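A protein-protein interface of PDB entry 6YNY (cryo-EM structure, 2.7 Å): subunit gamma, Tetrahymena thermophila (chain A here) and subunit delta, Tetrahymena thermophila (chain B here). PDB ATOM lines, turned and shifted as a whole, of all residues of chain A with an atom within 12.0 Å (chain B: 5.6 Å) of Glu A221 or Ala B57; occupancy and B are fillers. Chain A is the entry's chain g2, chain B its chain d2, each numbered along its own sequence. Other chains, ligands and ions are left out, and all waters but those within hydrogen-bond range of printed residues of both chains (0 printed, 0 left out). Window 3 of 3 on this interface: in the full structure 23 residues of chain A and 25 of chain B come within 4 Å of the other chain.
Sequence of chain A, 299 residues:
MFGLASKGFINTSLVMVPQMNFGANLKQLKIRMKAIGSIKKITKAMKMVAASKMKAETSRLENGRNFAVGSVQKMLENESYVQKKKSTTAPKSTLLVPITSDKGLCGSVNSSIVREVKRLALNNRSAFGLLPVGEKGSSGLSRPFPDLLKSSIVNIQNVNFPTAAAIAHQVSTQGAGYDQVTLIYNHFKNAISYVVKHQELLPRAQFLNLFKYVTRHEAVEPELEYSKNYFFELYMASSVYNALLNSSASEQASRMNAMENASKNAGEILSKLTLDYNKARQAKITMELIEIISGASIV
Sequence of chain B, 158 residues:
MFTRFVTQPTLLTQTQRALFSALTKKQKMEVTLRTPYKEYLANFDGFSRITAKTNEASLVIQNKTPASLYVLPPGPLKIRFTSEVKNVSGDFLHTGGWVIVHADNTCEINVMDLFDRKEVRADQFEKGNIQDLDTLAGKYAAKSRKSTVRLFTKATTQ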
ATOM      1  N   PHE A 211     -25.293 -24.837  14.736  1.00  0.00           N
ATOM      2  CA  PHE A 211     -24.978 -23.576  15.398  1.00  0.00           C
ATOM      3  C   PHE A 211     -24.975 -22.405  14.423  1.00  0.00           C
ATOM      4  O   PHE A 211     -25.287 -21.275  14.817  1.00  0.00           O
ATOM      5  CB  PHE A 211     -23.626 -23.683  16.101  1.00  0.00           C
ATOM      6  CG  PHE A 211     -23.412 -22.644  17.161  1.00  0.00           C
ATOM      7  CD1 PHE A 211     -23.861 -22.852  18.453  1.00  0.00           C
ATOM      8  CD2 PHE A 211     -22.758 -21.462  16.866  1.00  0.00           C
ATOM      9  CE1 PHE A 211     -23.666 -21.898  19.431  1.00  0.00           C
ATOM     10  CE2 PHE A 211     -22.559 -20.505  17.841  1.00  0.00           C
ATOM     11  CZ  PHE A 211     -23.012 -20.724  19.125  1.00  0.00           C
ATOM     12  N   VAL A 214     -27.832 -20.036  14.306  1.00  0.00           N
ATOM     13  CA  VAL A 214     -28.094 -19.160  15.441  1.00  0.00           C
ATOM     14  C   VAL A 214     -28.154 -17.719  14.961  1.00  0.00           C
ATOM     15  O   VAL A 214     -27.183 -17.191  14.406  1.00  0.00           O
ATOM     16  CB  VAL A 214     -27.026 -19.344  16.521  1.00  0.00           C
ATOM     17  CG1 VAL A 214     -27.165 -18.269  17.584  1.00  0.00           C
ATOM     18  CG2 VAL A 214     -27.132 -20.729  17.136  1.00  0.00           C
ATOM     19  N   HIS A 217     -29.507 -14.899  19.219  1.00  0.00           N
ATOM     20  CA  HIS A 217     -28.434 -14.481  20.113  1.00  0.00           C
ATOM     21  C   HIS A 217     -27.248 -14.045  19.261  1.00  0.00           C
ATOM     22  O   HIS A 217     -26.547 -14.882  18.683  1.00  0.00           O
ATOM     23  CB  HIS A 217     -28.045 -15.612  21.061  1.00  0.00           C
ATOM     24  CG  HIS A 217     -29.167 -16.093  21.930  1.00  0.00           C
ATOM     25  ND1 HIS A 217     -30.341 -16.601  21.419  1.00  0.00           N
ATOM     26  CD2 HIS A 217     -29.290 -16.147  23.278  1.00  0.00           C
ATOM     27  CE1 HIS A 217     -31.140 -16.945  22.413  1.00  0.00           C
ATOM     28  NE2 HIS A 217     -30.526 -16.680  23.552  1.00  0.00           N
ATOM     29  N   GLU A 218     -27.027 -12.737  19.176  1.00  0.00           N
ATOM     30  CA  GLU A 218     -25.954 -12.207  18.348  1.00  0.00           C
ATOM     31  C   GLU A 218     -24.589 -12.613  18.897  1.00  0.00           C
ATOM     32  O   GLU A 218     -24.383 -12.712  20.108  1.00  0.00           O
ATOM     33  CB  GLU A 218     -26.051 -10.684  18.269  1.00  0.00           C
ATOM     34  CG  GLU A 218     -25.017 -10.040  17.363  1.00  0.00           C
ATOM     35  CD  GLU A 218     -25.121  -8.528  17.341  1.00  0.00           C
ATOM     36  OE1 GLU A 218     -25.739  -7.962  18.266  1.00  0.00           O
ATOM     37  OE2 GLU A 218     -24.587  -7.907  16.398  1.00  0.00           O
ATOM     38  N   ALA A 219     -23.649 -12.848  17.979  1.00  0.00           N
ATOM     39  CA  ALA A 219     -22.269 -13.212  18.320  1.00  0.00           C
ATOM     40  C   ALA A 219     -21.356 -12.408  17.398  1.00  0.00           C
ATOM     41  O   ALA A 219     -21.057 -12.837  16.281  1.00  0.00           O
ATOM     42  CB  ALA A 219     -22.037 -14.709  18.178  1.00  0.00           C
ATOM     43  N   VAL A 220     -20.917 -11.242  17.871  1.00  0.00           N
ATOM     44  CA  VAL A 220     -20.077 -10.368  17.059  1.00  0.00           C
ATOM     45  C   VAL A 220     -18.773 -10.022  17.766  1.00  0.00           C
ATOM     46  O   VAL A 220     -17.764  -9.742  17.110  1.00  0.00           O
ATOM     47  CB  VAL A 220     -20.840  -9.090  16.675  1.00  0.00           C
ATOM     48  CG1 VAL A 220     -21.958  -9.427  15.708  1.00  0.00           C
ATOM     49  CG2 VAL A 220     -21.388  -8.402  17.914  1.00  0.00           C
ATOM     50  N   GLU A 221     -18.771 -10.029  19.102  1.00  0.00           N
ATOM     51  CA  GLU A 221     -17.514  -9.814  19.818  1.00  0.00           C
ATOM     52  C   GLU A 221     -16.472 -10.843  19.405  1.00  0.00           C
ATOM     53  O   GLU A 221     -15.426 -10.455  18.857  1.00  0.00           O
ATOM     54  CB  GLU A 221     -17.777  -9.802  21.326  1.00  0.00           C
ATOM     55  CG  GLU A 221     -18.483  -8.549  21.821  1.00  0.00           C
ATOM     56  CD  GLU A 221     -17.663  -7.291  21.616  1.00  0.00           C
ATOM     57  OE1 GLU A 221     -16.438  -7.407  21.401  1.00  0.00           O
ATOM     58  OE2 GLU A 221     -18.243  -6.186  21.670  1.00  0.00           O
ATOM     59  N   PRO A 222     -16.674 -12.142  19.628  1.00  0.00           N
ATOM     60  CA  PRO A 222     -15.999 -13.137  18.793  1.00  0.00           C
ATOM     61  C   PRO A 222     -16.900 -13.519  17.631  1.00  0.00           C
ATOM     62  O   PRO A 222     -18.108 -13.712  17.786  1.00  0.00           O
ATOM     63  CB  PRO A 222     -15.794 -14.307  19.761  1.00  0.00           C
ATOM     64  CG  PRO A 222     -16.983 -14.241  20.635  1.00  0.00           C
ATOM     65  CD  PRO A 222     -17.328 -12.775  20.787  1.00  0.00           C
ATOM     66  N   GLU A 223     -16.307 -13.626  16.448  1.00  0.00           N
ATOM     67  CA  GLU A 223     -17.116 -13.916  15.277  1.00  0.00           C
ATOM     68  C   GLU A 223     -17.664 -15.336  15.348  1.00  0.00           C
ATOM     69  O   GLU A 223     -17.140 -16.205  16.051  1.00  0.00           O
ATOM     70  CB  GLU A 223     -16.304 -13.716  13.999  1.00  0.00           C
ATOM     71  CG  GLU A 223     -15.966 -12.266  13.717  1.00  0.00           C
ATOM     72  CD  GLU A 223     -17.189 -11.441  13.369  1.00  0.00           C
ATOM     73  OE1 GLU A 223     -18.259 -12.038  13.122  1.00  0.00           O
ATOM     74  OE2 GLU A 223     -17.082 -10.198  13.345  1.00  0.00           O
ATOM     75  N   LEU A 224     -18.746 -15.564  14.601  1.00  0.00           N
ATOM     76  CA  LEU A 224     -19.456 -16.833  14.696  1.00  0.00           C
ATOM     77  C   LEU A 224     -18.537 -18.010  14.394  1.00  0.00           C
ATOM     78  O   LEU A 224     -18.660 -19.075  15.009  1.00  0.00           O
ATOM     79  CB  LEU A 224     -20.653 -16.830  13.748  1.00  0.00           C
ATOM     80  CG  LEU A 224     -21.584 -18.037  13.842  1.00  0.00           C
ATOM     81  CD1 LEU A 224     -22.164 -18.155  15.237  1.00  0.00           C
ATOM     82  CD2 LEU A 224     -22.695 -17.929  12.817  1.00  0.00           C
ATOM     83  N   GLU A 225     -17.610 -17.840  13.449  1.00  0.00           N
ATOM     84  CA  GLU A 225     -16.715 -18.939  13.102  1.00  0.00           C
ATOM     85  C   GLU A 225     -15.894 -19.391  14.302  1.00  0.00           C
ATOM     86  O   GLU A 225     -15.558 -20.575  14.411  1.00  0.00           O
ATOM     87  CB  GLU A 225     -15.793 -18.526  11.955  1.00  0.00           C
ATOM     88  CG  GLU A 225     -14.855 -17.381  12.289  1.00  0.00           C
ATOM     89  CD  GLU A 225     -14.033 -16.940  11.095  1.00  0.00           C
ATOM     90  OE1 GLU A 225     -14.029 -17.659  10.074  1.00  0.00           O
ATOM     91  OE2 GLU A 225     -13.389 -15.873  11.177  1.00  0.00           O
ATOM     92  N   TYR A 226     -15.563 -18.471  15.207  1.00  0.00           N
ATOM     93  CA  TYR A 226     -14.838 -18.826  16.420  1.00  0.00           C
ATOM     94  C   TYR A 226     -15.778 -19.239  17.543  1.00  0.00           C
ATOM     95  O   TYR A 226     -15.486 -20.184  18.282  1.00  0.00           O
ATOM     96  CB  TYR A 226     -13.979 -17.649  16.886  1.00  0.00           C
ATOM     97  CG  TYR A 226     -13.165 -17.004  15.792  1.00  0.00           C
ATOM     98  CD1 TYR A 226     -11.893 -17.458  15.483  1.00  0.00           C
ATOM     99  CD2 TYR A 226     -13.670 -15.935  15.071  1.00  0.00           C
ATOM    100  CE1 TYR A 226     -11.149 -16.866  14.484  1.00  0.00           C
ATOM    101  CE2 TYR A 226     -12.932 -15.336  14.070  1.00  0.00           C
ATOM    102  CZ  TYR A 226     -11.673 -15.806  13.780  1.00  0.00           C
ATOM    103  OH  TYR A 226     -10.932 -15.212  12.784  1.00  0.00           O
ATOM    104  N   SER A 227     -16.906 -18.540  17.683  1.00  0.00           N
ATOM    105  CA  SER A 227     -17.822 -18.824  18.781  1.00  0.00           C
ATOM    106  C   SER A 227     -18.430 -20.213  18.652  1.00  0.00           C
ATOM    107  O   SER A 227     -18.642 -20.900  19.657  1.00  0.00           O
ATOM    108  CB  SER A 227     -18.919 -17.764  18.827  1.00  0.00           C
ATOM    109  OG  SER A 227     -19.792 -17.982  19.919  1.00  0.00           O
ATOM    110  N   LYS A 228     -18.721 -20.643  17.422  1.00  0.00           N
ATOM    111  CA  LYS A 228     -19.349 -21.944  17.228  1.00  0.00           C
ATOM    112  C   LYS A 228     -18.467 -23.064  17.764  1.00  0.00           C
ATOM    113  O   LYS A 228     -18.962 -24.005  18.395  1.00  0.00           O
ATOM    114  CB  LYS A 228     -19.651 -22.156  15.746  1.00  0.00           C
ATOM    115  CG  LYS A 228     -18.416 -22.208  14.864  1.00  0.00           C
ATOM    116  CD  LYS A 228     -18.755 -21.949  13.405  1.00  0.00           C
ATOM    117  CE  LYS A 228     -19.691 -23.000  12.841  1.00  0.00           C
ATOM    118  NZ  LYS A 228     -20.025 -22.730  11.418  1.00  0.00           N
ATOM    119  N   TYR A 230     -15.971 -22.694  20.019  1.00  0.00           N
ATOM    120  CA  TYR A 230     -15.698 -22.510  21.440  1.00  0.00           C
ATOM    121  C   TYR A 230     -16.846 -23.044  22.287  1.00  0.00           C
ATOM    122  O   TYR A 230     -16.647 -23.890  23.166  1.00  0.00           O
ATOM    123  CB  TYR A 230     -15.449 -21.032  21.738  1.00  0.00           C
ATOM    124  CG  TYR A 230     -14.158 -20.478  21.174  1.00  0.00           C
ATOM    125  CD1 TYR A 230     -13.256 -21.291  20.502  1.00  0.00           C
ATOM    126  CD2 TYR A 230     -13.836 -19.138  21.327  1.00  0.00           C
ATOM    127  CE1 TYR A 230     -12.078 -20.785  19.993  1.00  0.00           C
ATOM    128  CE2 TYR A 230     -12.661 -18.623  20.822  1.00  0.00           C
ATOM    129  CZ  TYR A 230     -11.786 -19.449  20.158  1.00  0.00           C
ATOM    130  OH  TYR A 230     -10.614 -18.934  19.656  1.00  0.00           O
ATOM    131  N   PHE A 231     -18.063 -22.558  22.034  1.00  0.00           N
ATOM    132  CA  PHE A 231     -19.212 -23.012  22.806  1.00  0.00           C
ATOM    133  C   PHE A 231     -19.467 -24.502  22.633  1.00  0.00           C
ATOM    134  O   PHE A 231     -20.152 -25.103  23.467  1.00  0.00           O
ATOM    135  CB  PHE A 231     -20.455 -22.215  22.413  1.00  0.00           C
ATOM    136  CG  PHE A 231     -20.540 -20.872  23.075  1.00  0.00           C
ATOM    137  CD1 PHE A 231     -20.169 -19.726  22.397  1.00  0.00           C
ATOM    138  CD2 PHE A 231     -20.982 -20.758  24.381  1.00  0.00           C
ATOM    139  CE1 PHE A 231     -20.243 -18.491  23.008  1.00  0.00           C
ATOM    140  CE2 PHE A 231     -21.057 -19.525  24.995  1.00  0.00           C
ATOM    141  CZ  PHE A 231     -20.686 -18.390  24.308  1.00  0.00           C
ATOM    142  N   ALA B  52     -17.431  -5.967  31.292  1.00  0.00           N
ATOM    143  CA  ALA B  52     -16.311  -6.869  31.083  1.00  0.00           C
ATOM    144  C   ALA B  52     -15.586  -6.469  29.808  1.00  0.00           C
ATOM    145  O   ALA B  52     -16.045  -5.613  29.049  1.00  0.00           O
ATOM    146  CB  ALA B  52     -16.773  -8.326  31.010  1.00  0.00           C
ATOM    147  N   LYS B  53     -14.440  -7.105  29.580  1.00  0.00           N
ATOM    148  CA  LYS B  53     -13.594  -6.830  28.426  1.00  0.00           C
ATOM    149  C   LYS B  53     -13.577  -8.055  27.525  1.00  0.00           C
ATOM    150  O   LYS B  53     -13.191  -9.145  27.961  1.00  0.00           O
ATOM    151  CB  LYS B  53     -12.172  -6.470  28.857  1.00  0.00           C
ATOM    152  CG  LYS B  53     -11.994  -5.035  29.330  1.00  0.00           C
ATOM    153  CD  LYS B  53     -12.649  -4.797  30.680  1.00  0.00           C
ATOM    154  CE  LYS B  53     -12.365  -3.397  31.200  1.00  0.00           C
ATOM    155  NZ  LYS B  53     -10.906  -3.144  31.378  1.00  0.00           N
ATOM    156  N   THR B  54     -13.995  -7.872  26.277  1.00  0.00           N
ATOM    157  CA  THR B  54     -13.936  -8.912  25.267  1.00  0.00           C
ATOM    158  C   THR B  54     -12.673  -8.727  24.430  1.00  0.00           C
ATOM    159  O   THR B  54     -11.832  -7.868  24.710  1.00  0.00           O
ATOM    160  CB  THR B  54     -15.191  -8.886  24.395  1.00  0.00           C
ATOM    161  OG1 THR B  54     -15.171  -7.724  23.557  1.00  0.00           O
ATOM    162  CG2 THR B  54     -16.437  -8.859  25.256  1.00  0.00           C
ATOM    163  N   ASN B  55     -12.535  -9.543  23.386  1.00  0.00           N
ATOM    164  CA  ASN B  55     -11.366  -9.433  22.521  1.00  0.00           C
ATOM    165  C   ASN B  55     -11.351  -8.100  21.784  1.00  0.00           C
ATOM    166  O   ASN B  55     -10.301  -7.453  21.684  1.00  0.00           O
ATOM    167  CB  ASN B  55     -11.342 -10.595  21.529  1.00  0.00           C
ATOM    168  CG  ASN B  55     -12.625 -10.705  20.728  1.00  0.00           C
ATOM    169  OD1 ASN B  55     -13.422  -9.769  20.679  1.00  0.00           O
ATOM    170  ND2 ASN B  55     -12.832 -11.855  20.098  1.00  0.00           N
ATOM    171  N   GLU B  56     -12.501  -7.672  21.263  1.00  0.00           N
ATOM    172  CA  GLU B  56     -12.554  -6.430  20.503  1.00  0.00           C
ATOM    173  C   GLU B  56     -12.554  -5.211  21.419  1.00  0.00           C
ATOM    174  O   GLU B  56     -11.743  -4.295  21.244  1.00  0.00           O
ATOM    175  CB  GLU B  56     -13.791  -6.416  19.605  1.00  0.00           C
ATOM    176  CG  GLU B  56     -13.598  -7.111  18.269  1.00  0.00           C
ATOM    177  CD  GLU B  56     -14.818  -6.997  17.373  1.00  0.00           C
ATOM    178  OE1 GLU B  56     -15.891  -7.505  17.759  1.00  0.00           O
ATOM    179  OE2 GLU B  56     -14.704  -6.397  16.284  1.00  0.00           O
ATOM    180  N   ALA B  57     -13.454  -5.181  22.398  1.00  0.00           N
ATOM    181  CA  ALA B  57     -13.596  -4.017  23.262  1.00  0.00           C
ATOM    182  C   ALA B  57     -14.389  -4.413  24.500  1.00  0.00           C
ATOM    183  O   ALA B  57     -14.826  -5.557  24.646  1.00  0.00           O
ATOM    184  CB  ALA B  57     -14.272  -2.863  22.520  1.00  0.00           C
ATOM    185  N   SER B  58     -14.573  -3.445  25.393  1.00  0.00           N
ATOM    186  CA  SER B  58     -15.312  -3.670  26.625  1.00  0.00           C
ATOM    187  C   SER B  58     -16.807  -3.512  26.384  1.00  0.00           C
ATOM    188  O   SER B  58     -17.245  -2.593  25.688  1.00  0.00           O
ATOM    189  CB  SER B  58     -14.854  -2.694  27.707  1.00  0.00           C
ATOM    190  OG  SER B  58     -15.091  -1.353  27.316  1.00  0.00           O
ATOM    191  N   LEU B  59     -17.586  -4.415  26.969  1.00  0.00           N
ATOM    192  CA  LEU B  59     -19.037  -4.398  26.864  1.00  0.00           C
ATOM    193  C   LEU B  59     -19.648  -4.164  28.237  1.00  0.00           C
ATOM    194  O   LEU B  59     -18.986  -4.276  29.271  1.00  0.00           O
ATOM    195  CB  LEU B  59     -19.568  -5.708  26.269  1.00  0.00           C
ATOM    196  CG  LEU B  59     -19.729  -6.897  27.223  1.00  0.00           C
ATOM    197  CD1 LEU B  59     -20.212  -8.122  26.460  1.00  0.00           C
ATOM    198  CD2 LEU B  59     -18.437  -7.204  27.968  1.00  0.00           C
ATOM    199  N   LEU B  69     -24.287 -13.716  22.496  1.00  0.00           N
ATOM    200  CA  LEU B  69     -23.252 -14.563  23.067  1.00  0.00           C
ATOM    201  C   LEU B  69     -21.947 -13.789  23.170  1.00  0.00           C
ATOM    202  O   LEU B  69     -21.674 -12.887  22.374  1.00  0.00           O
ATOM    203  CB  LEU B  69     -23.020 -15.819  22.223  1.00  0.00           C
ATOM    204  CG  LEU B  69     -24.222 -16.713  21.933  1.00  0.00           C
ATOM    205  CD1 LEU B  69     -24.922 -16.270  20.669  1.00  0.00           C
ATOM    206  CD2 LEU B  69     -23.777 -18.156  21.815  1.00  0.00           C
ATOM    207  N   TYR B  70     -21.140 -14.151  24.164  1.00  0.00           N
ATOM    208  CA  TYR B  70     -19.838 -13.532  24.350  1.00  0.00           C
ATOM    209  C   TYR B  70     -18.874 -14.568  24.904  1.00  0.00           C
ATOM    210  O   TYR B  70     -19.277 -15.576  25.488  1.00  0.00           O
ATOM    211  CB  TYR B  70     -19.915 -12.318  25.280  1.00  0.00           C
ATOM    212  CG  TYR B  70     -20.914 -11.277  24.838  1.00  0.00           C
ATOM    213  CD1 TYR B  70     -20.541 -10.244  23.994  1.00  0.00           C
ATOM    214  CD2 TYR B  70     -22.233 -11.331  25.264  1.00  0.00           C
ATOM    215  CE1 TYR B  70     -21.452  -9.292  23.587  1.00  0.00           C
ATOM    216  CE2 TYR B  70     -23.149 -10.385  24.862  1.00  0.00           C
ATOM    217  CZ  TYR B  70     -22.755  -9.367  24.024  1.00  0.00           C
ATOM    218  OH  TYR B  70     -23.668  -8.421  23.621  1.00  0.00           O
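Of the 10 printed residues of chain B, 6 touch a printed residue of chain A.
Among the printed residues, 12 pairs touch across the chains.
Among the printed residues, no Asp or Glu carboxylate lies within 4 Å of a Lys or Arg side-chain nitrogen of the other chain.
Of chain B, only Thr B54, Asn B55, Glu B56, Ala B57 and Tyr B70 come within 4 Å of Glu A221.
Of chain A, only Glu A221 comes within 4 Å of Ala B57.
No residue of chain A comes within 4 Å of Ala B52.
No residue of chain A comes within 4 Å of Lys B53.
Of chain A, only Glu A221 comes within 4 Å of Thr B54.
No residue of chain A comes within 4 Å of Ser B58.
No residue of chain A comes within 4 Å of Leu B59.
Tyr B70 touches two residues of chain A.
Of the printed residues of chain B, His A217 touches Leu B69 (2.9 Å).
Printed residues of chain B within 4 Å of Phe A231: Leu B69 and Tyr B70.
Of the printed residues of chain B, Pro A222 touches Asn B55.
Of the printed residues of chain B, Phe A211 touches Leu B69 (3.8 Å).
Val A214 touches none of the printed residues of chain B.
Glu A223 touches none of the printed residues of chain B.
The nearest residue of chain A that does not touch Ala B57 is Pro A222 (8.2 Å).
The nearest printed residue of chain B that does not touch Phe A211 is Tyr B70 (8.5 Å).
CZ of Phe A211 touches CD2 of Leu B69, at 3.8 Å.
Leu B69 touches His A217.
Glu A221 touches Ala B57.
Tyr B70 touches Glu A221.
Pro A222 touches Asn B55.
CD2 of Leu B69 touches CE1 of Phe A231, 3.7 Å away.
O of Tyr B70 touches CZ of Phe A231, at 3.4 Å.
The side-chain hydroxyl (OG1) of Thr B54 sits at hydrogen-bond distance from the backbone carbonyl oxygen (O) of Ala B57 (2.4 Å).
OG1 of Thr B54 lies within hydrogen-bond range of OE1 of Glu A221, at 2.5 Å.
O of Val A220 sits close to OE1 of Glu B56, 3.0 Å away.
The backbone carbonyl oxygen (O) of Glu A218 is in hydrogen-bond range of the backbone NH (N) of Leu B69 (2.6 Å).
The side-chain amide oxygen of Asn B55 lies close to the backbone carbonyl oxygen of Glu A221, at 2.8 Å.
The side-chain carboxylate of Glu B56 lies close to the backbone carbonyl oxygen of Glu A221 (3.2 Å).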
